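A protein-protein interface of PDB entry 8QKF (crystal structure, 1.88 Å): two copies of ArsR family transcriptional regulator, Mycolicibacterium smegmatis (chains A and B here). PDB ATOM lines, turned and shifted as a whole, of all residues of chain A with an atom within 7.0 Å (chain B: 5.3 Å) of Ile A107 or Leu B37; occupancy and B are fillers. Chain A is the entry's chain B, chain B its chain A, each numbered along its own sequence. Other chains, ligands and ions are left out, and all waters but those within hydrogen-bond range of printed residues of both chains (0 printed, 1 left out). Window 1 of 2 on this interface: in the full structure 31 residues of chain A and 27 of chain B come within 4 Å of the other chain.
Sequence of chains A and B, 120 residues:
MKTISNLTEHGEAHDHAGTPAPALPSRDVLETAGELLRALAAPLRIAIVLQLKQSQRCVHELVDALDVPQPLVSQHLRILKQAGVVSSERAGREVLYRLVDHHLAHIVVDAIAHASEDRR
The guanidinium group (NH1) of Arg A38 is in hydrogen-bond range of the backbone carbonyl oxygen (O) of Ala B41, 3.1 Å away. ND1 of His A103 sits at hydrogen-bond distance from OD1 of Asp B110, 3.3 Å away.
Printed residues of chain B that touch a printed residue of chain A: Ala B33, Gly B34, Leu B36, Leu B37, Arg B38, Leu B40, Ala B41, Ile B107, Asp B110 and Ala B111. Hydrophobic or aromatic side chains of chain A that line the printed part of chain B: Leu A36, Leu A37, Ala A41, Ile A46, His A103, His A106, Ile A107 and Ile A112. Along chain A the printed residues that touch a printed residue of chain B span positions 34 to 112. Among the printed residues, no Asp or Glu carboxylate lies within 4 Å of a Lys or Arg side-chain nitrogen of the other chain.
The side-chain carboxylate (OD1) of Asp A101 sits at hydrogen-bond distance from the backbone NH (N) of His A103 (3.2 Å). The backbone carbonyl oxygen (O) of His A102 lies close to a ring nitrogen (ND1) of His A106.
Of the printed residues of chain B, Ile A107 touches Leu B37 (3.9 Å), Ile B107 (3.8 Å), Asp B110 (3.8 Å) and Ala B111 (3.8 Å). Leu B37 touches just these residues of chain A: Leu A37 (3.9 Å), Leu A40 (3.9 Å) and Ile A107 (3.9 Å). Of the printed residues of chain B, Gly A34 touches Ala B41 (3.7 Å). Printed residues of chain B within 4 Å of Ala A41: Gly B34 (3.2 Å). Of the printed residues of chain A, Ile B107 touches Leu A37, Ile A107, Asp A110 and Ala A111. Printed residues of chain B within 4 Å of Ala A111: Ala B33, Leu B36 and Ile B107. Printed residues of chain B within 4 Å of His A106: Asp B110 (3.6 Å). Val A49 touches none of the printed residues of chain B. The nearest printed residue of chain B that does not touch Ile A107 is Leu B36 (6.8 Å).
Gly A34 touches Ala B41, and with the chains exchanged Ala A41 touches Gly B34. Leu A37 touches Leu B40, and with the chains exchanged Leu A40 touches Leu B37. Leu A37 touches Ala B111, but with the chains exchanged Ala A111 does not touch Leu B37 (4.1 Å). Ile A107 touches Asp B110, and with the chains exchanged Asp A110 touches Ile B107. Of the 23 pairs that touch across the chains among the printed residues, 15 have their exchanged pair printed and touching as well.
Among the printed residues, pairs that only touch across the chains: Ala A41 with Gly B34, Arg A38 with Arg B38, Ile A112 with Ala B33, Ile A46 with Gly B34, His A106 with Asp B110, Gly A34 with Ala B41, Ile A107 with Ala B111, Leu A37 with Leu B40, Ile A107 with Asp B110, Leu A37 with Ala B41, Ile A107 with Ile B107, Leu A36 with Ala B111, Ala A111 with Ile B107, Ile A107 with Leu B37, Ala A111 with Leu B36, Leu A40 with Leu B37, Leu A37 with Ile B107, Leu A37 with Ala B111, Asp A110 with Ile B107, Leu A37 with Leu B37 and Ala A111 with Ala B33.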
ATOM      1  N   GLY A  34     -15.960 -25.814  32.644  1.00  0.00           N
ATOM      2  CA  GLY A  34     -16.569 -26.546  31.565  1.00  0.00           C
ATOM      3  C   GLY A  34     -17.412 -25.707  30.595  1.00  0.00           C
ATOM      4  O   GLY A  34     -17.296 -25.866  29.383  1.00  0.00           O
ATOM      5  N   LEU A  36     -16.978 -22.559  29.932  1.00  0.00           N
ATOM      6  CA  LEU A  36     -15.896 -21.787  29.205  1.00  0.00           C
ATOM      7  C   LEU A  36     -15.307 -22.539  28.038  1.00  0.00           C
ATOM      8  O   LEU A  36     -15.294 -22.059  26.851  1.00  0.00           O
ATOM      9  CB  LEU A  36     -14.805 -21.429  30.192  1.00  0.00           C
ATOM     10  CG  LEU A  36     -13.587 -20.707  29.621  1.00  0.00           C
ATOM     11  CD1 LEU A  36     -14.067 -19.327  29.184  1.00  0.00           C
ATOM     12  CD2 LEU A  36     -12.514 -20.585  30.669  1.00  0.00           C
ATOM     13  N   LEU A  37     -14.847 -23.758  28.350  1.00  0.00           N
ATOM     14  CA  LEU A  37     -14.333 -24.646  27.351  1.00  0.00           C
ATOM     15  C   LEU A  37     -15.329 -24.946  26.228  1.00  0.00           C
ATOM     16  O   LEU A  37     -14.919 -24.939  25.025  1.00  0.00           O
ATOM     17  CB  LEU A  37     -13.699 -25.903  27.973  1.00  0.00           C
ATOM     18  CG  LEU A  37     -12.489 -25.698  28.867  1.00  0.00           C
ATOM     19  CD1 LEU A  37     -12.036 -26.980  29.555  1.00  0.00           C
ATOM     20  CD2 LEU A  37     -11.319 -25.165  28.049  1.00  0.00           C
ATOM     21  N   ARG A  38     -16.611 -25.134  26.553  1.00  0.00           N
ATOM     22  CA  ARG A  38     -17.625 -25.342  25.491  1.00  0.00           C
ATOM     23  C   ARG A  38     -17.789 -24.097  24.588  1.00  0.00           C
ATOM     24  O   ARG A  38     -17.967 -24.214  23.380  1.00  0.00           O
ATOM     25  CB  ARG A  38     -19.014 -25.775  26.056  1.00  0.00           C
ATOM     26  CG  ARG A  38     -19.180 -27.289  26.118  1.00  0.00           C
ATOM     27  CD  ARG A  38     -20.552 -27.876  26.526  1.00  0.00           C
ATOM     28  NE  ARG A  38     -21.255 -27.094  27.524  1.00  0.00           N
ATOM     29  CZ  ARG A  38     -21.092 -27.154  28.854  1.00  0.00           C
ATOM     30  NH1 ARG A  38     -20.212 -27.992  29.442  1.00  0.00           N
ATOM     31  NH2 ARG A  38     -21.830 -26.345  29.619  1.00  0.00           N
ATOM     32  N   ALA A  39     -17.750 -22.911  25.184  1.00  0.00           N
ATOM     33  CA  ALA A  39     -17.874 -21.667  24.439  1.00  0.00           C
ATOM     34  C   ALA A  39     -16.681 -21.424  23.507  1.00  0.00           C
ATOM     35  O   ALA A  39     -16.805 -20.787  22.486  1.00  0.00           O
ATOM     36  CB  ALA A  39     -18.072 -20.506  25.420  1.00  0.00           C
ATOM     37  N   LEU A  40     -15.517 -21.934  23.836  1.00  0.00           N
ATOM     38  CA  LEU A  40     -14.370 -21.735  22.991  1.00  0.00           C
ATOM     39  C   LEU A  40     -14.238 -22.769  21.887  1.00  0.00           C
ATOM     40  O   LEU A  40     -13.346 -22.633  21.048  1.00  0.00           O
ATOM     41  CB  LEU A  40     -13.086 -21.784  23.823  1.00  0.00           C
ATOM     42  CG  LEU A  40     -12.796 -20.689  24.835  1.00  0.00           C
ATOM     43  CD1 LEU A  40     -11.671 -21.164  25.734  1.00  0.00           C
ATOM     44  CD2 LEU A  40     -12.415 -19.415  24.073  1.00  0.00           C
ATOM     45  N   ALA A  41     -15.034 -23.838  21.922  1.00  0.00           N
ATOM     46  CA  ALA A  41     -14.817 -24.978  21.028  1.00  0.00           C
ATOM     47  C   ALA A  41     -15.147 -24.708  19.501  1.00  0.00           C
ATOM     48  O   ALA A  41     -14.488 -25.253  18.616  1.00  0.00           O
ATOM     49  CB  ALA A  41     -15.495 -26.246  21.585  1.00  0.00           C
ATOM     50  N   ALA A  42     -16.057 -23.809  19.156  1.00  0.00           N
ATOM     51  CA  ALA A  42     -16.238 -23.500  17.710  1.00  0.00           C
ATOM     52  C   ALA A  42     -14.932 -23.036  16.963  1.00  0.00           C
ATOM     53  O   ALA A  42     -14.120 -22.248  17.486  1.00  0.00           O
ATOM     54  CB  ALA A  42     -17.359 -22.486  17.517  1.00  0.00           C
ATOM     55  N   ILE A  46     -12.084 -20.027  18.185  1.00  0.00           N
ATOM     56  CA  ILE A  46     -10.674 -20.167  18.325  1.00  0.00           C
ATOM     57  C   ILE A  46      -9.910 -19.152  17.456  1.00  0.00           C
ATOM     58  O   ILE A  46      -8.874 -18.607  17.886  1.00  0.00           O
ATOM     59  CB  ILE A  46     -10.256 -21.600  17.931  1.00  0.00           C
ATOM     60  CG1 ILE A  46     -10.714 -22.617  19.001  1.00  0.00           C
ATOM     61  CG2 ILE A  46      -8.759 -21.696  17.788  1.00  0.00           C
ATOM     62  CD1 ILE A  46     -10.826 -24.043  18.502  1.00  0.00           C
ATOM     63  N   VAL A  49     -10.042 -15.699  19.036  1.00  0.00           N
ATOM     64  CA  VAL A  49      -9.152 -15.606  20.158  1.00  0.00           C
ATOM     65  C   VAL A  49      -7.701 -15.474  19.739  1.00  0.00           C
ATOM     66  O   VAL A  49      -6.927 -14.710  20.344  1.00  0.00           O
ATOM     67  CB  VAL A  49      -9.383 -16.822  21.107  1.00  0.00           C
ATOM     68  CG1 VAL A  49      -8.296 -16.937  22.147  1.00  0.00           C
ATOM     69  CG2 VAL A  49     -10.721 -16.670  21.780  1.00  0.00           C
ATOM     70  N   ASP A 101      -8.625 -12.030  29.560  1.00  0.00           N
ATOM     71  CA  ASP A 101      -7.324 -12.302  30.246  1.00  0.00           C
ATOM     72  C   ASP A 101      -6.439 -13.197  29.360  1.00  0.00           C
ATOM     73  O   ASP A 101      -6.898 -13.712  28.342  1.00  0.00           O
ATOM     74  CB  ASP A 101      -7.542 -12.888  31.665  1.00  0.00           C
ATOM     75  CG  ASP A 101      -8.326 -14.243  31.653  1.00  0.00           C
ATOM     76  OD1 ASP A 101      -8.062 -15.086  30.780  1.00  0.00           O
ATOM     77  OD2 ASP A 101      -9.215 -14.477  32.505  1.00  0.00           O
ATOM     78  N   HIS A 102      -5.203 -13.429  29.787  1.00  0.00           N
ATOM     79  CA  HIS A 102      -4.233 -14.320  29.088  1.00  0.00           C
ATOM     80  C   HIS A 102      -4.490 -15.833  29.236  1.00  0.00           C
ATOM     81  O   HIS A 102      -4.014 -16.612  28.421  1.00  0.00           O
ATOM     82  CB  HIS A 102      -2.792 -14.074  29.603  1.00  0.00           C
ATOM     83  CG  HIS A 102      -2.235 -12.727  29.252  1.00  0.00           C
ATOM     84  ND1 HIS A 102      -2.172 -11.687  30.160  1.00  0.00           N
ATOM     85  CD2 HIS A 102      -1.714 -12.249  28.097  1.00  0.00           C
ATOM     86  CE1 HIS A 102      -1.641 -10.627  29.577  1.00  0.00           C
ATOM     87  NE2 HIS A 102      -1.352 -10.943  28.326  1.00  0.00           N
ATOM     88  N   HIS A 103      -5.169 -16.249  30.310  1.00  0.00           N
ATOM     89  CA  HIS A 103      -5.546 -17.677  30.488  1.00  0.00           C
ATOM     90  C   HIS A 103      -6.237 -18.199  29.222  1.00  0.00           C
ATOM     91  O   HIS A 103      -5.982 -19.295  28.765  1.00  0.00           O
ATOM     92  CB  HIS A 103      -6.533 -17.887  31.674  1.00  0.00           C
ATOM     93  CG  HIS A 103      -5.978 -17.533  33.015  1.00  0.00           C
ATOM     94  ND1 HIS A 103      -4.803 -18.075  33.504  1.00  0.00           N
ATOM     95  CD2 HIS A 103      -6.437 -16.686  33.970  1.00  0.00           C
ATOM     96  CE1 HIS A 103      -4.563 -17.577  34.701  1.00  0.00           C
ATOM     97  NE2 HIS A 103      -5.542 -16.742  35.009  1.00  0.00           N
ATOM     98  N   LEU A 104      -7.072 -17.363  28.635  1.00  0.00           N
ATOM     99  CA  LEU A 104      -7.827 -17.724  27.442  1.00  0.00           C
ATOM    100  C   LEU A 104      -6.974 -17.982  26.180  1.00  0.00           C
ATOM    101  O   LEU A 104      -7.245 -18.894  25.375  1.00  0.00           O
ATOM    102  CB  LEU A 104      -8.880 -16.633  27.187  1.00  0.00           C
ATOM    103  CG  LEU A 104      -9.838 -16.450  28.381  1.00  0.00           C
ATOM    104  CD1 LEU A 104     -10.541 -15.106  28.383  1.00  0.00           C
ATOM    105  CD2 LEU A 104     -10.869 -17.576  28.368  1.00  0.00           C
ATOM    106  N   ALA A 105      -5.943 -17.175  25.975  1.00  0.00           N
ATOM    107  CA  ALA A 105      -5.100 -17.382  24.846  1.00  0.00           C
ATOM    108  C   ALA A 105      -4.279 -18.641  25.032  1.00  0.00           C
ATOM    109  O   ALA A 105      -4.120 -19.386  24.072  1.00  0.00           O
ATOM    110  CB  ALA A 105      -4.197 -16.166  24.623  1.00  0.00           C
ATOM    111  N   HIS A 106      -3.770 -18.871  26.242  1.00  0.00           N
ATOM    112  CA  HIS A 106      -3.016 -20.098  26.530  1.00  0.00           C
ATOM    113  C   HIS A 106      -3.843 -21.353  26.258  1.00  0.00           C
ATOM    114  O   HIS A 106      -3.322 -22.336  25.781  1.00  0.00           O
ATOM    115  CB  HIS A 106      -2.535 -20.125  27.968  1.00  0.00           C
ATOM    116  CG  HIS A 106      -1.631 -18.987  28.301  1.00  0.00           C
ATOM    117  ND1 HIS A 106      -1.475 -18.511  29.586  1.00  0.00           N
ATOM    118  CD2 HIS A 106      -0.856 -18.206  27.508  1.00  0.00           C
ATOM    119  CE1 HIS A 106      -0.623 -17.499  29.573  1.00  0.00           C
ATOM    120  NE2 HIS A 106      -0.232 -17.299  28.326  1.00  0.00           N
ATOM    121  N   ILE A 107      -5.127 -21.317  26.579  1.00  0.00           N
ATOM    122  CA  ILE A 107      -6.004 -22.464  26.357  1.00  0.00           C
ATOM    123  C   ILE A 107      -6.036 -22.791  24.869  1.00  0.00           C
ATOM    124  O   ILE A 107      -5.887 -23.945  24.458  1.00  0.00           O
ATOM    125  CB  ILE A 107      -7.450 -22.177  26.852  1.00  0.00           C
ATOM    126  CG1 ILE A 107      -7.525 -22.217  28.379  1.00  0.00           C
ATOM    127  CG2 ILE A 107      -8.401 -23.214  26.288  1.00  0.00           C
ATOM    128  CD1 ILE A 107      -8.758 -21.584  28.923  1.00  0.00           C
ATOM    129  N   VAL A 108      -6.258 -21.766  24.057  1.00  0.00           N
ATOM    130  CA  VAL A 108      -6.450 -21.926  22.612  1.00  0.00           C
ATOM    131  C   VAL A 108      -5.145 -22.295  21.946  1.00  0.00           C
ATOM    132  O   VAL A 108      -5.100 -23.171  21.087  1.00  0.00           O
ATOM    133  CB  VAL A 108      -7.039 -20.619  22.041  1.00  0.00           C
ATOM    134  CG1 VAL A 108      -6.629 -20.398  20.618  1.00  0.00           C
ATOM    135  CG2 VAL A 108      -8.549 -20.612  22.247  1.00  0.00           C
ATOM    136  N   VAL A 109      -4.080 -21.642  22.374  1.00  0.00           N
ATOM    137  CA  VAL A 109      -2.741 -21.910  21.829  1.00  0.00           C
ATOM    138  C   VAL A 109      -2.271 -23.356  22.147  1.00  0.00           C
ATOM    139  O   VAL A 109      -1.691 -24.019  21.286  1.00  0.00           O
ATOM    140  CB  VAL A 109      -1.756 -20.824  22.335  1.00  0.00           C
ATOM    141  CG1 VAL A 109      -0.303 -21.237  22.248  1.00  0.00           C
ATOM    142  CG2 VAL A 109      -1.973 -19.540  21.540  1.00  0.00           C
ATOM    143  N   ASP A 110      -2.554 -23.874  23.348  1.00  0.00           N
ATOM    144  CA  ASP A 110      -2.188 -25.268  23.681  1.00  0.00           C
ATOM    145  C   ASP A 110      -3.058 -26.285  22.959  1.00  0.00           C
ATOM    146  O   ASP A 110      -2.617 -27.354  22.563  1.00  0.00           O
ATOM    147  CB  ASP A 110      -2.234 -25.487  25.182  1.00  0.00           C
ATOM    148  CG  ASP A 110      -1.253 -24.561  25.960  1.00  0.00           C
ATOM    149  OD1 ASP A 110      -0.465 -23.797  25.322  1.00  0.00           O
ATOM    150  OD2 ASP A 110      -1.308 -24.573  27.225  1.00  0.00           O
ATOM    151  N   ALA A 111      -4.326 -25.956  22.791  1.00  0.00           N
ATOM    152  CA  ALA A 111      -5.189 -26.813  21.965  1.00  0.00           C
ATOM    153  C   ALA A 111      -4.689 -26.905  20.508  1.00  0.00           C
ATOM    154  O   ALA A 111      -4.660 -27.993  19.970  1.00  0.00           O
ATOM    155  CB  ALA A 111      -6.630 -26.314  21.997  1.00  0.00           C
ATOM    156  N   ILE A 112      -4.362 -25.755  19.878  1.00  0.00           N
ATOM    157  CA  ILE A 112      -3.785 -25.703  18.524  1.00  0.00           C
ATOM    158  C   ILE A 112      -2.498 -26.543  18.449  1.00  0.00           C
ATOM    159  O   ILE A 112      -2.332 -27.341  17.529  1.00  0.00           O
ATOM    160  CB  ILE A 112      -3.439 -24.254  18.065  1.00  0.00           C
ATOM    161  CG1 ILE A 112      -4.663 -23.355  17.942  1.00  0.00           C
ATOM    162  CG2 ILE A 112      -2.692 -24.233  16.720  1.00  0.00           C
ATOM    163  CD1 ILE A 112      -5.814 -23.924  17.198  1.00  0.00           C
ATOM    164  N   THR B  32     -10.005 -29.851  14.811  1.00  0.00           N
ATOM    165  CA  THR B  32      -9.403 -30.790  15.744  1.00  0.00           C
ATOM    166  C   THR B  32      -9.167 -30.128  17.114  1.00  0.00           C
ATOM    167  O   THR B  32      -9.462 -30.696  18.184  1.00  0.00           O
ATOM    168  CB  THR B  32      -8.066 -31.280  15.161  1.00  0.00           C
ATOM    169  OG1 THR B  32      -8.338 -32.012  13.978  1.00  0.00           O
ATOM    170  CG2 THR B  32      -7.296 -32.186  16.124  1.00  0.00           C
ATOM    171  N   ALA B  33      -8.645 -28.912  17.090  1.00  0.00           N
ATOM    172  CA  ALA B  33      -8.580 -28.080  18.316  1.00  0.00           C
ATOM    173  C   ALA B  33      -9.964 -27.930  18.974  1.00  0.00           C
ATOM    174  O   ALA B  33     -10.122 -28.158  20.183  1.00  0.00           O
ATOM    175  CB  ALA B  33      -7.898 -26.734  18.020  1.00  0.00           C
ATOM    176  N   GLY B  34     -10.992 -27.643  18.185  1.00  0.00           N
ATOM    177  CA  GLY B  34     -12.354 -27.581  18.683  1.00  0.00           C
ATOM    178  C   GLY B  34     -12.851 -28.833  19.393  1.00  0.00           C
ATOM    179  O   GLY B  34     -13.494 -28.773  20.473  1.00  0.00           O
ATOM    180  N   GLU B  35     -12.584 -29.978  18.785  1.00  0.00           N
ATOM    181  CA  GLU B  35     -12.999 -31.266  19.388  1.00  0.00           C
ATOM    182  C   GLU B  35     -12.241 -31.589  20.676  1.00  0.00           C
ATOM    183  O   GLU B  35     -12.778 -32.186  21.578  1.00  0.00           O
ATOM    184  CB  GLU B  35     -12.739 -32.396  18.397  1.00  0.00           C
ATOM    185  CG  GLU B  35     -13.450 -32.205  17.072  1.00  0.00           C
ATOM    186  CD  GLU B  35     -13.337 -33.452  16.196  1.00  0.00           C
ATOM    187  OE1 GLU B  35     -14.346 -33.797  15.512  1.00  0.00           O
ATOM    188  OE2 GLU B  35     -12.246 -34.096  16.212  1.00  0.00           O
ATOM    189  N   LEU B  36     -10.955 -31.262  20.706  1.00  0.00           N
ATOM    190  CA  LEU B  36     -10.169 -31.411  21.886  1.00  0.00           C
ATOM    191  C   LEU B  36     -10.811 -30.621  23.050  1.00  0.00           C
ATOM    192  O   LEU B  36     -11.074 -31.197  24.127  1.00  0.00           O
ATOM    193  CB  LEU B  36      -8.736 -30.998  21.627  1.00  0.00           C
ATOM    194  CG  LEU B  36      -7.842 -31.042  22.841  1.00  0.00           C
ATOM    195  CD1 LEU B  36      -7.709 -32.501  23.272  1.00  0.00           C
ATOM    196  CD2 LEU B  36      -6.477 -30.431  22.530  1.00  0.00           C
ATOM    197  N   LEU B  37     -11.202 -29.374  22.809  1.00  0.00           N
ATOM    198  CA  LEU B  37     -11.791 -28.523  23.892  1.00  0.00           C
ATOM    199  C   LEU B  37     -13.144 -29.039  24.358  1.00  0.00           C
ATOM    200  O   LEU B  37     -13.496 -28.999  25.545  1.00  0.00           O
ATOM    201  CB  LEU B  37     -11.921 -27.062  23.461  1.00  0.00           C
ATOM    202  CG  LEU B  37     -10.601 -26.343  23.278  1.00  0.00           C
ATOM    203  CD1 LEU B  37     -10.718 -24.925  22.755  1.00  0.00           C
ATOM    204  CD2 LEU B  37      -9.784 -26.377  24.571  1.00  0.00           C
ATOM    205  N   ARG B  38     -13.879 -29.588  23.428  1.00  0.00           N
ATOM    206  CA  ARG B  38     -15.189 -30.104  23.750  1.00  0.00           C
ATOM    207  C   ARG B  38     -15.057 -31.416  24.551  1.00  0.00           C
ATOM    208  O   ARG B  38     -15.781 -31.657  25.472  1.00  0.00           O
ATOM    209  CB  ARG B  38     -15.946 -30.220  22.440  1.00  0.00           C
ATOM    210  CG  ARG B  38     -17.290 -30.841  22.523  1.00  0.00           C
ATOM    211  CD  ARG B  38     -18.358 -29.898  23.039  1.00  0.00           C
ATOM    212  NE  ARG B  38     -19.534 -30.735  23.284  1.00  0.00           N
ATOM    213  CZ  ARG B  38     -20.796 -30.332  23.373  1.00  0.00           C
ATOM    214  NH1 ARG B  38     -21.129 -29.044  23.266  1.00  0.00           N
ATOM    215  NH2 ARG B  38     -21.732 -31.256  23.581  1.00  0.00           N
ATOM    216  N   ALA B  39     -14.052 -32.211  24.254  1.00  0.00           N
ATOM    217  CA  ALA B  39     -13.711 -33.402  25.066  1.00  0.00           C
ATOM    218  C   ALA B  39     -13.301 -33.087  26.505  1.00  0.00           C
ATOM    219  O   ALA B  39     -13.534 -33.879  27.442  1.00  0.00           O
ATOM    220  CB  ALA B  39     -12.594 -34.199  24.373  1.00  0.00           C
ATOM    221  N   LEU B  40     -12.667 -31.940  26.716  1.00  0.00           N
ATOM    222  CA  LEU B  40     -12.250 -31.526  28.056  1.00  0.00           C
ATOM    223  C   LEU B  40     -13.338 -30.790  28.862  1.00  0.00           C
ATOM    224  O   LEU B  40     -13.161 -30.547  30.029  1.00  0.00           O
ATOM    225  CB  LEU B  40     -11.036 -30.605  27.928  1.00  0.00           C
ATOM    226  CG  LEU B  40      -9.752 -31.227  27.416  1.00  0.00           C
ATOM    227  CD1 LEU B  40      -8.731 -30.145  27.123  1.00  0.00           C
ATOM    228  CD2 LEU B  40      -9.188 -32.223  28.438  1.00  0.00           C
ATOM    229  N   ALA B  41     -14.457 -30.446  28.220  1.00  0.00           N
ATOM    230  CA  ALA B  41     -15.421 -29.502  28.715  1.00  0.00           C
ATOM    231  C   ALA B  41     -16.527 -30.129  29.528  1.00  0.00           C
ATOM    232  O   ALA B  41     -17.692 -29.870  29.253  1.00  0.00           O
ATOM    233  CB  ALA B  41     -16.069 -28.869  27.538  1.00  0.00           C
ATOM    234  N   ILE B 107      -4.534 -26.795  29.931  1.00  0.00           N
ATOM    235  CA  ILE B 107      -5.823 -26.307  29.438  1.00  0.00           C
ATOM    236  C   ILE B 107      -6.848 -26.251  30.557  1.00  0.00           C
ATOM    237  O   ILE B 107      -7.511 -25.226  30.742  1.00  0.00           O
ATOM    238  CB  ILE B 107      -6.337 -27.114  28.217  1.00  0.00           C
ATOM    239  CG1 ILE B 107      -5.403 -26.877  27.053  1.00  0.00           C
ATOM    240  CG2 ILE B 107      -7.741 -26.682  27.810  1.00  0.00           C
ATOM    241  CD1 ILE B 107      -5.600 -27.813  25.920  1.00  0.00           C
ATOM    242  N   ASP B 110      -5.837 -23.618  33.393  1.00  0.00           N
ATOM    243  CA  ASP B 110      -6.148 -22.251  32.945  1.00  0.00           C
ATOM    244  C   ASP B 110      -7.648 -21.950  32.896  1.00  0.00           C
ATOM    245  O   ASP B 110      -8.048 -20.833  33.221  1.00  0.00           O
ATOM    246  CB  ASP B 110      -5.511 -22.002  31.572  1.00  0.00           C
ATOM    247  CG  ASP B 110      -3.968 -21.770  31.647  1.00  0.00           C
ATOM    248  OD1 ASP B 110      -3.572 -20.995  32.545  1.00  0.00           O
ATOM    249  OD2 ASP B 110      -3.181 -22.312  30.790  1.00  0.00           O
ATOM    250  N   ALA B 111      -8.465 -22.917  32.437  1.00  0.00           N
ATOM    251  CA  ALA B 111      -9.915 -22.797  32.452  1.00  0.00           C
ATOM    252  C   ALA B 111     -10.421 -22.590  33.876  1.00  0.00           C
ATOM    253  O   ALA B 111     -11.292 -21.751  34.107  1.00  0.00           O
ATOM    254  CB  ALA B 111     -10.566 -24.022  31.836  1.00  0.00           C
